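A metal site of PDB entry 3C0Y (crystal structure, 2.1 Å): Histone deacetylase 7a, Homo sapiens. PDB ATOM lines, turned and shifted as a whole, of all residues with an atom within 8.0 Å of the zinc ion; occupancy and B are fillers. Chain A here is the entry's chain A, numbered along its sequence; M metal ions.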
ATOM      1  N   GLN A  52      13.759 -23.845  20.764  1.00  0.00           N
ATOM      2  CA  GLN A  52      12.691 -23.959  21.760  1.00  0.00           C
ATOM      3  C   GLN A  52      13.341 -24.316  23.061  1.00  0.00           C
ATOM      4  O   GLN A  52      14.239 -25.144  23.101  1.00  0.00           O
ATOM      5  CB  GLN A  52      11.654 -25.067  21.408  1.00  0.00           C
ATOM      6  CG  GLN A  52      11.249 -25.157  19.919  1.00  0.00           C
ATOM      7  CD  GLN A  52      10.341 -26.347  19.590  1.00  0.00           C
ATOM      8  OE1 GLN A  52       9.123 -26.199  19.417  1.00  0.00           O
ATOM      9  NE2 GLN A  52      10.928 -27.534  19.505  1.00  0.00           N
ATOM     10  N   CYS A  53      12.877 -23.708  24.142  1.00  0.00           N
ATOM     11  CA  CYS A  53      13.336 -24.125  25.453  1.00  0.00           C
ATOM     12  C   CYS A  53      13.064 -25.617  25.674  1.00  0.00           C
ATOM     13  O   CYS A  53      12.082 -26.206  25.123  1.00  0.00           O
ATOM     14  CB  CYS A  53      12.688 -23.302  26.559  1.00  0.00           C
ATOM     15  SG  CYS A  53      13.543 -23.513  28.173  1.00  0.00           S
ATOM     16  N   SER A  54      13.902 -26.223  26.507  1.00  0.00           N
ATOM     17  CA  SER A  54      13.691 -27.634  26.874  1.00  0.00           C
ATOM     18  C   SER A  54      12.591 -27.890  27.941  1.00  0.00           C
ATOM     19  O   SER A  54      12.216 -29.060  28.170  1.00  0.00           O
ATOM     20  CB  SER A  54      15.003 -28.221  27.329  1.00  0.00           C
ATOM     21  OG  SER A  54      15.530 -27.335  28.272  1.00  0.00           O
ATOM     22  N   CYS A  55      12.114 -26.811  28.605  1.00  0.00           N
ATOM     23  CA  CYS A  55      10.936 -26.850  29.511  1.00  0.00           C
ATOM     24  C   CYS A  55       9.645 -27.194  28.768  1.00  0.00           C
ATOM     25  O   CYS A  55       8.699 -27.680  29.387  1.00  0.00           O
ATOM     26  CB  CYS A  55      10.741 -25.534  30.260  1.00  0.00           C
ATOM     27  SG  CYS A  55       9.814 -24.280  29.329  1.00  0.00           S
ATOM     28  N   GLY A  56       9.620 -26.958  27.459  1.00  0.00           N
ATOM     29  CA  GLY A  56       8.513 -27.374  26.578  1.00  0.00           C
ATOM     30  C   GLY A  56       7.179 -26.671  26.824  1.00  0.00           C
ATOM     31  O   GLY A  56       6.125 -27.292  26.718  1.00  0.00           O
ATOM     32  N   ASP A  57       7.241 -25.380  27.151  1.00  0.00           N
ATOM     33  CA  ASP A  57       6.070 -24.595  27.566  1.00  0.00           C
ATOM     34  C   ASP A  57       6.081 -23.188  26.960  1.00  0.00           C
ATOM     35  O   ASP A  57       6.732 -22.269  27.477  1.00  0.00           O
ATOM     36  CB  ASP A  57       6.006 -24.500  29.099  1.00  0.00           C
ATOM     37  CG  ASP A  57       4.728 -23.779  29.597  1.00  0.00           C
ATOM     38  OD1 ASP A  57       3.722 -23.712  28.816  1.00  0.00           O
ATOM     39  OD2 ASP A  57       4.727 -23.285  30.746  1.00  0.00           O
ATOM     40  N   ASN A  58       5.343 -23.029  25.862  1.00  0.00           N
ATOM     41  CA  ASN A  58       5.226 -21.760  25.155  1.00  0.00           C
ATOM     42  C   ASN A  58       4.652 -20.586  25.962  1.00  0.00           C
ATOM     43  O   ASN A  58       4.760 -19.438  25.523  1.00  0.00           O
ATOM     44  CB  ASN A  58       4.381 -21.961  23.905  1.00  0.00           C
ATOM     45  CG  ASN A  58       5.105 -22.707  22.814  1.00  0.00           C
ATOM     46  OD1 ASN A  58       6.247 -23.147  22.988  1.00  0.00           O
ATOM     47  ND2 ASN A  58       4.454 -22.841  21.649  1.00  0.00           N
ATOM     48  N   ARG A  60       5.569 -19.386  28.983  1.00  0.00           N
ATOM     49  CA  ARG A  60       6.562 -18.480  29.570  1.00  0.00           C
ATOM     50  C   ARG A  60       7.609 -17.997  28.571  1.00  0.00           C
ATOM     51  O   ARG A  60       8.603 -17.394  28.965  1.00  0.00           O
ATOM     52  CB  ARG A  60       7.208 -19.031  30.848  1.00  0.00           C
ATOM     53  CG  ARG A  60       7.652 -20.462  30.833  1.00  0.00           C
ATOM     54  CD  ARG A  60       7.806 -20.973  32.262  1.00  0.00           C
ATOM     55  NE  ARG A  60       7.706 -22.420  32.372  1.00  0.00           N
ATOM     56  CZ  ARG A  60       7.586 -23.081  33.521  1.00  0.00           C
ATOM     57  NH1 ARG A  60       7.538 -22.404  34.660  1.00  0.00           N
ATOM     58  NH2 ARG A  60       7.530 -24.407  33.526  1.00  0.00           N
ATOM     59  N   HIS A  61       7.369 -18.274  27.293  1.00  0.00           N
ATOM     60  CA  HIS A  61       8.376 -18.065  26.223  1.00  0.00           C
ATOM     61  C   HIS A  61       7.715 -17.542  24.964  1.00  0.00           C
ATOM     62  O   HIS A  61       7.492 -18.318  24.013  1.00  0.00           O
ATOM     63  CB  HIS A  61       9.110 -19.367  25.867  1.00  0.00           C
ATOM     64  CG  HIS A  61       9.883 -19.956  27.001  1.00  0.00           C
ATOM     65  ND1 HIS A  61      10.752 -19.225  27.783  1.00  0.00           N
ATOM     66  CD2 HIS A  61       9.953 -21.233  27.451  1.00  0.00           C
ATOM     67  CE1 HIS A  61      11.292 -20.016  28.691  1.00  0.00           C
ATOM     68  NE2 HIS A  61      10.823 -21.237  28.516  1.00  0.00           N
ATOM     69  N   LEU A 136      17.476 -21.104  33.907  1.00  0.00           N
ATOM     70  CA  LEU A 136      16.204 -20.387  33.930  1.00  0.00           C
ATOM     71  C   LEU A 136      15.333 -20.967  35.053  1.00  0.00           C
ATOM     72  O   LEU A 136      15.557 -22.090  35.496  1.00  0.00           O
ATOM     73  CB  LEU A 136      15.502 -20.450  32.549  1.00  0.00           C
ATOM     74  CG  LEU A 136      16.341 -19.811  31.431  1.00  0.00           C
ATOM     75  CD1 LEU A 136      15.706 -20.004  30.076  1.00  0.00           C
ATOM     76  CD2 LEU A 136      16.682 -18.342  31.675  1.00  0.00           C
ATOM     77  N   PRO A 137      14.375 -20.163  35.551  1.00  0.00           N
ATOM     78  CA  PRO A 137      13.395 -20.631  36.534  1.00  0.00           C
ATOM     79  C   PRO A 137      12.685 -21.909  36.092  1.00  0.00           C
ATOM     80  O   PRO A 137      12.328 -22.716  36.938  1.00  0.00           O
ATOM     81  CB  PRO A 137      12.404 -19.463  36.626  1.00  0.00           C
ATOM     82  CG  PRO A 137      13.284 -18.225  36.355  1.00  0.00           C
ATOM     83  CD  PRO A 137      14.194 -18.721  35.242  1.00  0.00           C
ATOM     84  N   CYS A 138      12.528 -22.097  34.772  1.00  0.00           N
ATOM     85  CA  CYS A 138      11.882 -23.302  34.223  1.00  0.00           C
ATOM     86  C   CYS A 138      12.844 -24.481  34.124  1.00  0.00           C
ATOM     87  O   CYS A 138      12.435 -25.580  33.699  1.00  0.00           O
ATOM     88  CB  CYS A 138      11.289 -22.989  32.861  1.00  0.00           C
ATOM     89  SG  CYS A 138      12.517 -22.488  31.538  1.00  0.00           S
ATOM     90  N   GLY A 139      14.106 -24.254  34.505  1.00  0.00           N
ATOM     91  CA  GLY A 139      15.197 -25.255  34.405  1.00  0.00           C
ATOM     92  C   GLY A 139      15.937 -25.443  33.058  1.00  0.00           C
ATOM     93  O   GLY A 139      16.878 -26.253  32.955  1.00  0.00           O
ATOM     94  N   GLY A 140      15.533 -24.687  32.043  1.00  0.00           N
ATOM     95  CA  GLY A 140      16.187 -24.740  30.752  1.00  0.00           C
ATOM     96  C   GLY A 140      17.333 -23.763  30.803  1.00  0.00           C
ATOM     97  O   GLY A 140      17.396 -22.907  31.705  1.00  0.00           O
ATOM     98  N   VAL A 141      18.221 -23.870  29.833  1.00  0.00           N
ATOM     99  CA  VAL A 141      19.397 -23.015  29.776  1.00  0.00           C
ATOM    100  C   VAL A 141      18.981 -21.732  29.076  1.00  0.00           C
ATOM    101  O   VAL A 141      18.114 -21.761  28.207  1.00  0.00           O
ATOM    102  CB  VAL A 141      20.525 -23.731  29.038  1.00  0.00           C
ATOM    103  CG1 VAL A 141      21.749 -22.790  28.755  1.00  0.00           C
ATOM    104  CG2 VAL A 141      20.931 -24.900  29.828  1.00  0.00           C
ATOM    105  N   THR A 145      17.178 -14.302  31.493  1.00  0.00           N
ATOM    106  CA  THR A 145      15.838 -14.905  31.809  1.00  0.00           C
ATOM    107  C   THR A 145      14.955 -15.118  30.588  1.00  0.00           C
ATOM    108  O   THR A 145      14.269 -16.161  30.462  1.00  0.00           O
ATOM    109  CB  THR A 145      15.044 -14.125  32.881  1.00  0.00           C
ATOM    110  OG1 THR A 145      15.109 -12.735  32.599  1.00  0.00           O
ATOM    111  CG2 THR A 145      15.627 -14.382  34.289  1.00  0.00           C
ATOM    112  N   ILE A 148      16.386 -17.727  25.607  1.00  0.00           N
ATOM    113  CA  ILE A 148      16.577 -19.120  25.894  1.00  0.00           C
ATOM    114  C   ILE A 148      17.637 -19.686  24.933  1.00  0.00           C
ATOM    115  O   ILE A 148      17.881 -19.120  23.876  1.00  0.00           O
ATOM    116  CB  ILE A 148      15.223 -19.925  25.798  1.00  0.00           C
ATOM    117  CG1 ILE A 148      14.786 -20.158  24.345  1.00  0.00           C
ATOM    118  CG2 ILE A 148      14.102 -19.185  26.569  1.00  0.00           C
ATOM    119  CD1 ILE A 148      15.293 -21.494  23.682  1.00  0.00           C
HETATM  120 ZN    ZN M   1      11.602 -22.809  29.555  1.00  0.00          ZN
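The side-chain sulfur of Cys 55 sits close to the backbone NH of Asp 57.
The side-chain sulfur of Cys 138 lies close to the backbone NH of Gly 140 (3.8 Å).
Within 4 Å of the zinc ion: Cys 53, Cys 55, His 61 and Cys 138.
The zinc ion is bound by a ring nitrogen (NE2) of His 61, the side-chain sulfur (SG) of Cys 138, the side-chain sulfur (SG) of Cys 55 and the side-chain sulfur (SG) of Cys 53.
The zinc ion has four donor atoms within binding distance.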
